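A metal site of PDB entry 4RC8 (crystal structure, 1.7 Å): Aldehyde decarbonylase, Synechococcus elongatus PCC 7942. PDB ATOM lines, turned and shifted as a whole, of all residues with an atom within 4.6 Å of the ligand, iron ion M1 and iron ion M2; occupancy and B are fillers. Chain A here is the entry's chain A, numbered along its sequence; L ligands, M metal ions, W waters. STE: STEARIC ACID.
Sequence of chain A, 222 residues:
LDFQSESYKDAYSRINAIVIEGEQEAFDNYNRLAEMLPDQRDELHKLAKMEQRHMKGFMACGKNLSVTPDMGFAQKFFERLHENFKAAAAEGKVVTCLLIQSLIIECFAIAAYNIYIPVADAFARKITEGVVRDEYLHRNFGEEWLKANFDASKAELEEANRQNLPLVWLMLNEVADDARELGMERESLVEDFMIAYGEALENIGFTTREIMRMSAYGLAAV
Water W2 lies within hydrogen-bond range of the side-chain carboxylate (OE2) of Glu 23 (2.5 Å) and the side-chain carboxylate (OE2) of Glu 135 (2.7 Å).
Tyr 12 touches the ligand (OH to C18, 3.1 Å).
Ile 15 touches the ligand (CG2 to C15, 3.8 Å).
Asn 16 touches the ligand (ND2 to C18, 3.4 Å).
Ile 18 touches the ligand.
Val 19 touches the ligand (CG2 to C18, 3.4 Å).
O of Gly 22 touches C2 of the ligand, at 3.9 Å.
Ala 26 touches the ligand.
CE1 of Phe 58 touches C16 of the ligand, 3.6 Å away.
Ile 105 touches the ligand (CG2 to C2, 3.4 Å).
Phe 108 touches the ligand (CE2 to C8, 3.6 Å).
Ala 112 touches the ligand.
Tyr 113 touches the ligand (OH to C5, 3.4 Å).
Tyr 116 touches the ligand (CE2 to C17, 3.4 Å).
Met 184 touches the ligand (CE to C13, 3.7 Å).
Hydrophobic or aromatic side chains within 4 Å of the ligand: Tyr 12, Ile 15, Ile 18, Val 19, Ala 26, Phe 58, Ile 105, Phe 108, Ala 112, Tyr 113, Tyr 116 and Met 184.
Of the 27 residues printed, 18 come within 4 Å of the ligand.
The nearest printed residue that does not touch the ligand is Glu 135 (4.1 Å).
Iron ion M1 is bound by water W1, water W2, the side-chain carboxylate (OE1) of Glu 51, the side-chain carboxylate (OE1) of Glu 23, an oxygen (O2) of the ligand and a ring nitrogen (ND1) of His 54.
Of the 27 residues printed, 3 come within 4 Å of iron ion M2.
The nearest printed residue that does not touch iron ion M2 is Gln 101 (4.1 Å).
Iron ion M2 is bound by water W1 (1.9 Å), the side-chain carboxylate (OE2) of Glu 51 (2.0 Å), the side-chain carboxylate (OE2) of Glu 106 (2.1 Å), a ring nitrogen (ND1) of His 138 (2.3 Å), an oxygen (O1) of the ligand (2.3 Å) and the side-chain carboxylate (OE1) of Glu 106 (2.4 Å).
Iron ion M2 has six donor atoms within binding distance.
An oxygen (O1) of the ligand sits close to the side-chain amide nitrogen (NE2) of Gln 101 (3.0 Å).
Within 4 Å of iron ion M1: Glu 23, Glu 51 and His 54.
The nearest printed residue that does not touch iron ion M1 is Glu 135 (4.3 Å).
The side-chain carboxylate (OE2) of Glu 23 lies within hydrogen-bond range of the side-chain hydroxyl (OH) of Tyr 113, at 2.7 Å.
N of Glu 106 sits close to O of Gln 101, at 3.2 Å.
OH of Tyr 30 lies close to OE2 of Glu 106, 2.8 Å away.
OH of Tyr 12 sits at hydrogen-bond distance from OH of Tyr 116, 2.9 Å away.
The backbone carbonyl oxygen (O) of Phe 58 lies within hydrogen-bond range of the side-chain amide nitrogen (ND2) of Asn 16 (2.8 Å).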
ATOM      1  N   TYR A  12      16.370 -24.246  30.479  1.00  0.00           N
ATOM      2  CA  TYR A  12      16.393 -23.423  29.281  1.00  0.00           C
ATOM      3  C   TYR A  12      16.503 -21.929  29.615  1.00  0.00           C
ATOM      4  O   TYR A  12      17.122 -21.177  28.866  1.00  0.00           O
ATOM      5  CB  TYR A  12      15.177 -23.682  28.369  1.00  0.00           C
ATOM      6  CG  TYR A  12      15.478 -23.432  26.903  1.00  0.00           C
ATOM      7  CD1 TYR A  12      16.093 -24.405  26.127  1.00  0.00           C
ATOM      8  CD2 TYR A  12      15.136 -22.219  26.297  1.00  0.00           C
ATOM      9  CE1 TYR A  12      16.381 -24.189  24.776  1.00  0.00           C
ATOM     10  CE2 TYR A  12      15.418 -21.990  24.950  1.00  0.00           C
ATOM     11  CZ  TYR A  12      16.037 -22.974  24.195  1.00  0.00           C
ATOM     12  OH  TYR A  12      16.316 -22.761  22.873  1.00  0.00           O
ATOM     13  N   ILE A  15      20.271 -21.496  30.007  1.00  0.00           N
ATOM     14  CA  ILE A  15      20.974 -21.760  28.732  1.00  0.00           C
ATOM     15  C   ILE A  15      20.688 -20.705  27.664  1.00  0.00           C
ATOM     16  O   ILE A  15      21.611 -20.202  27.015  1.00  0.00           O
ATOM     17  CB  ILE A  15      20.635 -23.167  28.157  1.00  0.00           C
ATOM     18  CG1 ILE A  15      21.020 -24.274  29.136  1.00  0.00           C
ATOM     19  CG2 ILE A  15      21.312 -23.391  26.800  1.00  0.00           C
ATOM     20  CD1 ILE A  15      22.493 -24.420  29.367  1.00  0.00           C
ATOM     21  N   ASN A  16      19.406 -20.383  27.468  1.00  0.00           N
ATOM     22  CA  ASN A  16      18.994 -19.346  26.533  1.00  0.00           C
ATOM     23  C   ASN A  16      19.643 -18.001  26.869  1.00  0.00           C
ATOM     24  O   ASN A  16      20.154 -17.324  25.990  1.00  0.00           O
ATOM     25  CB  ASN A  16      17.451 -19.244  26.516  1.00  0.00           C
ATOM     26  CG  ASN A  16      16.931 -18.280  25.476  1.00  0.00           C
ATOM     27  OD1 ASN A  16      16.186 -17.348  25.803  1.00  0.00           O
ATOM     28  ND2 ASN A  16      17.310 -18.491  24.218  1.00  0.00           N
ATOM     29  N   ILE A  18      22.445 -17.592  28.528  1.00  0.00           N
ATOM     30  CA  ILE A  18      23.875 -17.735  28.260  1.00  0.00           C
ATOM     31  C   ILE A  18      24.176 -17.497  26.778  1.00  0.00           C
ATOM     32  O   ILE A  18      25.119 -16.765  26.444  1.00  0.00           O
ATOM     33  CB  ILE A  18      24.430 -19.092  28.744  1.00  0.00           C
ATOM     34  CG1 ILE A  18      24.615 -19.074  30.267  1.00  0.00           C
ATOM     35  CG2 ILE A  18      25.745 -19.433  28.050  1.00  0.00           C
ATOM     36  CD1 ILE A  18      24.874 -20.458  30.857  1.00  0.00           C
ATOM     37  N   VAL A  19      23.401 -18.108  25.890  1.00  0.00           N
ATOM     38  CA  VAL A  19      23.670 -17.916  24.471  1.00  0.00           C
ATOM     39  C   VAL A  19      23.350 -16.506  23.991  1.00  0.00           C
ATOM     40  O   VAL A  19      24.103 -15.954  23.204  1.00  0.00           O
ATOM     41  CB  VAL A  19      23.024 -18.999  23.545  1.00  0.00           C
ATOM     42  CG1 VAL A  19      23.573 -20.374  23.891  1.00  0.00           C
ATOM     43  CG2 VAL A  19      21.524 -18.968  23.610  1.00  0.00           C
ATOM     44  N   GLY A  22      26.231 -14.394  25.182  1.00  0.00           N
ATOM     45  CA  GLY A  22      27.431 -14.725  24.419  1.00  0.00           C
ATOM     46  C   GLY A  22      27.452 -14.085  23.047  1.00  0.00           C
ATOM     47  O   GLY A  22      28.489 -13.586  22.602  1.00  0.00           O
ATOM     48  N   GLU A  23      26.307 -14.096  22.371  1.00  0.00           N
ATOM     49  CA  GLU A  23      26.178 -13.475  21.056  1.00  0.00           C
ATOM     50  C   GLU A  23      26.323 -11.956  21.153  1.00  0.00           C
ATOM     51  O   GLU A  23      26.940 -11.331  20.300  1.00  0.00           O
ATOM     52  CB  GLU A  23      24.833 -13.821  20.394  1.00  0.00           C
ATOM     53  CG  GLU A  23      24.516 -15.315  20.256  1.00  0.00           C
ATOM     54  CD  GLU A  23      25.443 -16.062  19.306  1.00  0.00           C
ATOM     55  OE1 GLU A  23      26.191 -15.421  18.539  1.00  0.00           O
ATOM     56  OE2 GLU A  23      25.409 -17.316  19.316  1.00  0.00           O
ATOM     57  N   ALA A  26      29.883 -11.210  21.697  1.00  0.00           N
ATOM     58  CA  ALA A  26      30.630 -11.430  20.464  1.00  0.00           C
ATOM     59  C   ALA A  26      30.467 -10.252  19.487  1.00  0.00           C
ATOM     60  O   ALA A  26      31.421  -9.859  18.821  1.00  0.00           O
ATOM     61  CB  ALA A  26      30.203 -12.725  19.815  1.00  0.00           C
ATOM     62  N   TYR A  30      33.794  -8.259  18.264  1.00  0.00           N
ATOM     63  CA  TYR A  30      34.216  -8.091  16.871  1.00  0.00           C
ATOM     64  C   TYR A  30      34.219  -6.626  16.454  1.00  0.00           C
ATOM     65  O   TYR A  30      35.102  -6.222  15.705  1.00  0.00           O
ATOM     66  CB  TYR A  30      33.406  -8.963  15.911  1.00  0.00           C
ATOM     67  CG  TYR A  30      33.807 -10.426  15.973  1.00  0.00           C
ATOM     68  CD1 TYR A  30      35.125 -10.821  15.741  1.00  0.00           C
ATOM     69  CD2 TYR A  30      32.866 -11.406  16.247  1.00  0.00           C
ATOM     70  CE1 TYR A  30      35.497 -12.164  15.811  1.00  0.00           C
ATOM     71  CE2 TYR A  30      33.216 -12.752  16.320  1.00  0.00           C
ATOM     72  CZ  TYR A  30      34.531 -13.117  16.091  1.00  0.00           C
ATOM     73  OH  TYR A  30      34.889 -14.452  16.167  1.00  0.00           O
ATOM     74  N   GLU A  51      26.733 -11.718  14.494  1.00  0.00           N
ATOM     75  CA  GLU A  51      26.485 -11.965  15.918  1.00  0.00           C
ATOM     76  C   GLU A  51      25.174 -11.327  16.378  1.00  0.00           C
ATOM     77  O   GLU A  51      24.430 -11.922  17.159  1.00  0.00           O
ATOM     78  CB  GLU A  51      27.653 -11.487  16.786  1.00  0.00           C
ATOM     79  CG  GLU A  51      29.000 -12.085  16.396  1.00  0.00           C
ATOM     80  CD  GLU A  51      29.103 -13.569  16.698  1.00  0.00           C
ATOM     81  OE1 GLU A  51      28.073 -14.203  17.021  1.00  0.00           O
ATOM     82  OE2 GLU A  51      30.226 -14.111  16.639  1.00  0.00           O
ATOM     83  N   HIS A  54      22.487 -13.612  15.254  1.00  0.00           N
ATOM     84  CA  HIS A  54      22.429 -14.784  16.142  1.00  0.00           C
ATOM     85  C   HIS A  54      21.703 -14.464  17.437  1.00  0.00           C
ATOM     86  O   HIS A  54      20.866 -15.255  17.892  1.00  0.00           O
ATOM     87  CB  HIS A  54      23.825 -15.292  16.509  1.00  0.00           C
ATOM     88  CG  HIS A  54      24.681 -15.646  15.339  1.00  0.00           C
ATOM     89  ND1 HIS A  54      26.036 -15.876  15.461  1.00  0.00           N
ATOM     90  CD2 HIS A  54      24.383 -15.813  14.027  1.00  0.00           C
ATOM     91  CE1 HIS A  54      26.530 -16.167  14.265  1.00  0.00           C
ATOM     92  NE2 HIS A  54      25.555 -16.129  13.379  1.00  0.00           N
ATOM     93  N   PHE A  58      18.307 -16.354  18.900  1.00  0.00           N
ATOM     94  CA  PHE A  58      18.186 -17.056  20.171  1.00  0.00           C
ATOM     95  C   PHE A  58      17.169 -16.414  21.116  1.00  0.00           C
ATOM     96  O   PHE A  58      16.554 -17.099  21.928  1.00  0.00           O
ATOM     97  CB  PHE A  58      19.559 -17.238  20.828  1.00  0.00           C
ATOM     98  CG  PHE A  58      20.428 -18.252  20.116  1.00  0.00           C
ATOM     99  CD1 PHE A  58      19.937 -19.516  19.813  1.00  0.00           C
ATOM    100  CD2 PHE A  58      21.724 -17.929  19.739  1.00  0.00           C
ATOM    101  CE1 PHE A  58      20.720 -20.453  19.144  1.00  0.00           C
ATOM    102  CE2 PHE A  58      22.521 -18.867  19.071  1.00  0.00           C
ATOM    103  CZ  PHE A  58      22.016 -20.123  18.775  1.00  0.00           C
ATOM    104  N   CYS A  61      14.099 -18.039  20.093  1.00  0.00           N
ATOM    105  CA  CYS A  61      14.036 -19.410  20.604  1.00  0.00           C
ATOM    106  C   CYS A  61      13.428 -19.460  22.010  1.00  0.00           C
ATOM    107  O   CYS A  61      12.619 -20.345  22.308  1.00  0.00           O
ATOM    108  CB  CYS A  61      15.420 -20.056  20.621  1.00  0.00           C
ATOM    109  SG  CYS A  61      16.093 -20.416  18.989  1.00  0.00           S
ATOM    110  N   PHE A  78      29.694 -15.130  32.060  1.00  0.00           N
ATOM    111  CA  PHE A  78      30.690 -14.605  31.123  1.00  0.00           C
ATOM    112  C   PHE A  78      31.691 -13.606  31.724  1.00  0.00           C
ATOM    113  O   PHE A  78      32.709 -13.306  31.105  1.00  0.00           O
ATOM    114  CB  PHE A  78      29.986 -13.939  29.940  1.00  0.00           C
ATOM    115  CG  PHE A  78      29.612 -14.896  28.845  1.00  0.00           C
ATOM    116  CD1 PHE A  78      30.568 -15.326  27.924  1.00  0.00           C
ATOM    117  CD2 PHE A  78      28.306 -15.360  28.721  1.00  0.00           C
ATOM    118  CE1 PHE A  78      30.240 -16.215  26.901  1.00  0.00           C
ATOM    119  CE2 PHE A  78      27.972 -16.243  27.694  1.00  0.00           C
ATOM    120  CZ  PHE A  78      28.927 -16.672  26.797  1.00  0.00           C
ATOM    121  N   GLN A 101      37.966 -14.484  21.582  1.00  0.00           N
ATOM    122  CA  GLN A 101      36.734 -14.586  20.852  1.00  0.00           C
ATOM    123  C   GLN A 101      36.728 -15.566  19.663  1.00  0.00           C
ATOM    124  O   GLN A 101      35.865 -16.364  19.563  1.00  0.00           O
ATOM    125  CB  GLN A 101      36.313 -13.207  20.334  1.00  0.00           C
ATOM    126  CG  GLN A 101      35.035 -13.187  19.472  1.00  0.00           C
ATOM    127  CD  GLN A 101      33.779 -13.691  20.181  1.00  0.00           C
ATOM    128  OE1 GLN A 101      33.487 -13.292  21.250  1.00  0.00           O
ATOM    129  NE2 GLN A 101      33.065 -14.653  19.519  1.00  0.00           N
ATOM    130  N   ILE A 105      36.195 -18.984  22.299  1.00  0.00           N
ATOM    131  CA  ILE A 105      34.739 -18.872  22.374  1.00  0.00           C
ATOM    132  C   ILE A 105      34.040 -19.514  21.165  1.00  0.00           C
ATOM    133  O   ILE A 105      33.065 -20.249  21.349  1.00  0.00           O
ATOM    134  CB  ILE A 105      34.295 -17.411  22.608  1.00  0.00           C
ATOM    135  CG1 ILE A 105      34.633 -17.015  24.045  1.00  0.00           C
ATOM    136  CG2 ILE A 105      32.802 -17.263  22.363  1.00  0.00           C
ATOM    137  CD1 ILE A 105      34.425 -15.517  24.346  1.00  0.00           C
ATOM    138  N   GLU A 106      34.517 -19.250  19.951  1.00  0.00           N
ATOM    139  CA  GLU A 106      33.869 -19.868  18.773  1.00  0.00           C
ATOM    140  C   GLU A 106      33.965 -21.381  18.818  1.00  0.00           C
ATOM    141  O   GLU A 106      33.021 -22.066  18.453  1.00  0.00           O
ATOM    142  CB  GLU A 106      34.429 -19.353  17.435  1.00  0.00           C
ATOM    143  CG  GLU A 106      34.354 -17.841  17.199  1.00  0.00           C
ATOM    144  CD  GLU A 106      32.962 -17.299  16.933  1.00  0.00           C
ATOM    145  OE1 GLU A 106      32.012 -18.083  16.671  1.00  0.00           O
ATOM    146  OE2 GLU A 106      32.804 -16.065  16.970  1.00  0.00           O
ATOM    147  N   PHE A 108      34.112 -23.286  21.541  1.00  0.00           N
ATOM    148  CA  PHE A 108      33.186 -23.699  22.579  1.00  0.00           C
ATOM    149  C   PHE A 108      31.771 -23.700  22.003  1.00  0.00           C
ATOM    150  O   PHE A 108      31.024 -24.668  22.175  1.00  0.00           O
ATOM    151  CB  PHE A 108      33.343 -22.760  23.796  1.00  0.00           C
ATOM    152  CG  PHE A 108      32.498 -23.118  24.992  1.00  0.00           C
ATOM    153  CD1 PHE A 108      32.273 -24.441  25.353  1.00  0.00           C
ATOM    154  CD2 PHE A 108      31.958 -22.106  25.787  1.00  0.00           C
ATOM    155  CE1 PHE A 108      31.504 -24.753  26.473  1.00  0.00           C
ATOM    156  CE2 PHE A 108      31.197 -22.408  26.910  1.00  0.00           C
ATOM    157  CZ  PHE A 108      30.965 -23.737  27.252  1.00  0.00           C
ATOM    158  N   ALA A 109      31.432 -22.651  21.260  1.00  0.00           N
ATOM    159  CA  ALA A 109      30.106 -22.518  20.666  1.00  0.00           C
ATOM    160  C   ALA A 109      29.836 -23.547  19.573  1.00  0.00           C
ATOM    161  O   ALA A 109      28.749 -24.123  19.508  1.00  0.00           O
ATOM    162  CB  ALA A 109      29.918 -21.111  20.121  1.00  0.00           C
ATOM    163  N   ALA A 112      29.280 -26.894  21.363  1.00  0.00           N
ATOM    164  CA  ALA A 112      28.009 -26.936  22.078  1.00  0.00           C
ATOM    165  C   ALA A 112      26.804 -26.882  21.148  1.00  0.00           C
ATOM    166  O   ALA A 112      25.848 -27.638  21.323  1.00  0.00           O
ATOM    167  CB  ALA A 112      27.934 -25.825  23.127  1.00  0.00           C
ATOM    168  N   TYR A 113      26.836 -25.992  20.152  1.00  0.00           N
ATOM    169  CA  TYR A 113      25.691 -25.820  19.281  1.00  0.00           C
ATOM    170  C   TYR A 113      25.440 -27.077  18.444  1.00  0.00           C
ATOM    171  O   TYR A 113      24.288 -27.455  18.223  1.00  0.00           O
ATOM    172  CB  TYR A 113      25.843 -24.590  18.395  1.00  0.00           C
ATOM    173  CG  TYR A 113      25.737 -23.237  19.100  1.00  0.00           C
ATOM    174  CD1 TYR A 113      25.721 -23.130  20.494  1.00  0.00           C
ATOM    175  CD2 TYR A 113      25.678 -22.066  18.356  1.00  0.00           C
ATOM    176  CE1 TYR A 113      25.635 -21.887  21.134  1.00  0.00           C
ATOM    177  CE2 TYR A 113      25.594 -20.818  18.979  1.00  0.00           C
ATOM    178  CZ  TYR A 113      25.570 -20.734  20.353  1.00  0.00           C
ATOM    179  OH  TYR A 113      25.501 -19.489  20.952  1.00  0.00           O
ATOM    180  N   TYR A 116      23.655 -29.517  20.593  1.00  0.00           N
ATOM    181  CA  TYR A 116      22.267 -29.087  20.773  1.00  0.00           C
ATOM    182  C   TYR A 116      21.371 -29.452  19.592  1.00  0.00           C
ATOM    183  O   TYR A 116      20.228 -29.862  19.792  1.00  0.00           O
ATOM    184  CB  TYR A 116      22.221 -27.578  21.010  1.00  0.00           C
ATOM    185  CG  TYR A 116      20.847 -26.981  21.185  1.00  0.00           C
ATOM    186  CD1 TYR A 116      19.967 -27.461  22.159  1.00  0.00           C
ATOM    187  CD2 TYR A 116      20.436 -25.907  20.399  1.00  0.00           C
ATOM    188  CE1 TYR A 116      18.704 -26.891  22.327  1.00  0.00           C
ATOM    189  CE2 TYR A 116      19.188 -25.328  20.558  1.00  0.00           C
ATOM    190  CZ  TYR A 116      18.329 -25.822  21.531  1.00  0.00           C
ATOM    191  OH  TYR A 116      17.095 -25.250  21.684  1.00  0.00           O
ATOM    192  N   VAL A 131      23.096 -20.527  12.632  1.00  0.00           N
ATOM    193  CA  VAL A 131      24.107 -19.885  13.475  1.00  0.00           C
ATOM    194  C   VAL A 131      25.462 -20.591  13.388  1.00  0.00           C
ATOM    195  O   VAL A 131      26.484 -19.938  13.203  1.00  0.00           O
ATOM    196  CB  VAL A 131      23.640 -19.792  14.956  1.00  0.00           C
ATOM    197  CG1 VAL A 131      24.750 -19.254  15.829  1.00  0.00           C
ATOM    198  CG2 VAL A 131      22.395 -18.923  15.078  1.00  0.00           C
ATOM    199  N   GLU A 135      29.535 -19.592  12.598  1.00  0.00           N
ATOM    200  CA  GLU A 135      30.600 -19.818  13.578  1.00  0.00           C
ATOM    201  C   GLU A 135      31.854 -20.406  12.928  1.00  0.00           C
ATOM    202  O   GLU A 135      32.966 -20.066  13.333  1.00  0.00           O
ATOM    203  CB  GLU A 135      30.137 -20.698  14.731  1.00  0.00           C
ATOM    204  CG  GLU A 135      29.064 -20.042  15.577  1.00  0.00           C
ATOM    205  CD  GLU A 135      28.611 -20.900  16.725  1.00  0.00           C
ATOM    206  OE1 GLU A 135      28.686 -22.156  16.619  1.00  0.00           O
ATOM    207  OE2 GLU A 135      28.172 -20.327  17.749  1.00  0.00           O
ATOM    208  N   HIS A 138      33.739 -17.574  11.537  1.00  0.00           N
ATOM    209  CA  HIS A 138      34.363 -16.761  12.588  1.00  0.00           C
ATOM    210  C   HIS A 138      35.658 -17.398  13.057  1.00  0.00           C
ATOM    211  O   HIS A 138      36.691 -16.732  13.143  1.00  0.00           O
ATOM    212  CB  HIS A 138      33.419 -16.548  13.768  1.00  0.00           C
ATOM    213  CG  HIS A 138      32.163 -15.824  13.406  1.00  0.00           C
ATOM    214  ND1 HIS A 138      31.121 -15.641  14.295  1.00  0.00           N
ATOM    215  CD2 HIS A 138      31.752 -15.265  12.236  1.00  0.00           C
ATOM    216  CE1 HIS A 138      30.152 -14.983  13.698  1.00  0.00           C
ATOM    217  NE2 HIS A 138      30.501 -14.740  12.452  1.00  0.00           N
ATOM    218  N   VAL A 175      27.877 -25.107  33.253  1.00  0.00           N
ATOM    219  CA  VAL A 175      26.711 -25.276  32.396  1.00  0.00           C
ATOM    220  C   VAL A 175      26.276 -26.743  32.253  1.00  0.00           C
ATOM    221  O   VAL A 175      25.167 -27.034  31.783  1.00  0.00           O
ATOM    222  CB  VAL A 175      26.966 -24.609  30.997  1.00  0.00           C
ATOM    223  CG1 VAL A 175      27.710 -25.561  30.048  1.00  0.00           C
ATOM    224  CG2 VAL A 175      25.669 -24.125  30.393  1.00  0.00           C
ATOM    225  N   MET A 184      21.969 -32.698  26.345  1.00  0.00           N
ATOM    226  CA  MET A 184      23.344 -32.534  25.888  1.00  0.00           C
ATOM    227  C   MET A 184      24.335 -33.123  26.876  1.00  0.00           C
ATOM    228  O   MET A 184      24.521 -32.590  27.980  1.00  0.00           O
ATOM    229  CB  MET A 184      23.655 -31.051  25.690  1.00  0.00           C
ATOM    230  CG  MET A 184      22.764 -30.347  24.686  1.00  0.00           C
ATOM    231  SD  MET A 184      22.962 -28.566  24.791  1.00  0.00           S
ATOM    232  CE  MET A 184      24.712 -28.388  24.403  1.00  0.00           C
HETATM  233  C1  STE L   1      29.625 -16.470  19.446  1.00  0.00           C
HETATM  234  O1  STE L   1      30.641 -16.213  18.772  1.00  0.00           O
HETATM  235  O2  STE L   1      28.485 -16.449  18.949  1.00  0.00           O
HETATM  236  C2  STE L   1      29.799 -16.809  20.908  1.00  0.00           C
HETATM  237  C3  STE L   1      28.550 -17.482  21.534  1.00  0.00           C
HETATM  238  C4  STE L   1      28.921 -18.079  22.887  1.00  0.00           C
HETATM  239  C5  STE L   1      27.821 -18.997  23.398  1.00  0.00           C
HETATM  240  C6  STE L   1      28.392 -20.097  24.302  1.00  0.00           C
HETATM  241  C7  STE L   1      27.271 -21.032  24.776  1.00  0.00           C
HETATM  242  C8  STE L   1      27.765 -22.033  25.821  1.00  0.00           C
HETATM  243  C9  STE L   1      26.601 -22.705  26.547  1.00  0.00           C
HETATM  244  C10 STE L   1      26.495 -24.223  26.116  1.00  0.00           C
HETATM  245  C11 STE L   1      24.970 -24.586  25.944  1.00  0.00           C
HETATM  246  C12 STE L   1      24.460 -23.993  24.610  1.00  0.00           C
HETATM  247  C13 STE L   1      23.435 -24.927  23.958  1.00  0.00           C
HETATM  248  C14 STE L   1      22.826 -24.277  22.721  1.00  0.00           C
HETATM  249  C15 STE L   1      21.445 -23.701  23.040  1.00  0.00           C
HETATM  250  C16 STE L   1      21.131 -22.468  22.075  1.00  0.00           C
HETATM  251  C17 STE L   1      19.509 -22.369  22.153  1.00  0.00           C
HETATM  252  C18 STE L   1      19.008 -21.192  23.096  1.00  0.00           C
HETATM  253 FE    FE M   1      27.513 -16.125  17.137  1.00  0.00          FE
HETATM  254 FE    FE M   2      30.723 -16.088  16.467  1.00  0.00          FE
HETATM  255  O   HOH W   1      28.925 -16.668  16.142  1.00  0.00           O
HETATM  256  O   HOH W   2      26.942 -17.953  17.473  1.00  0.00           O
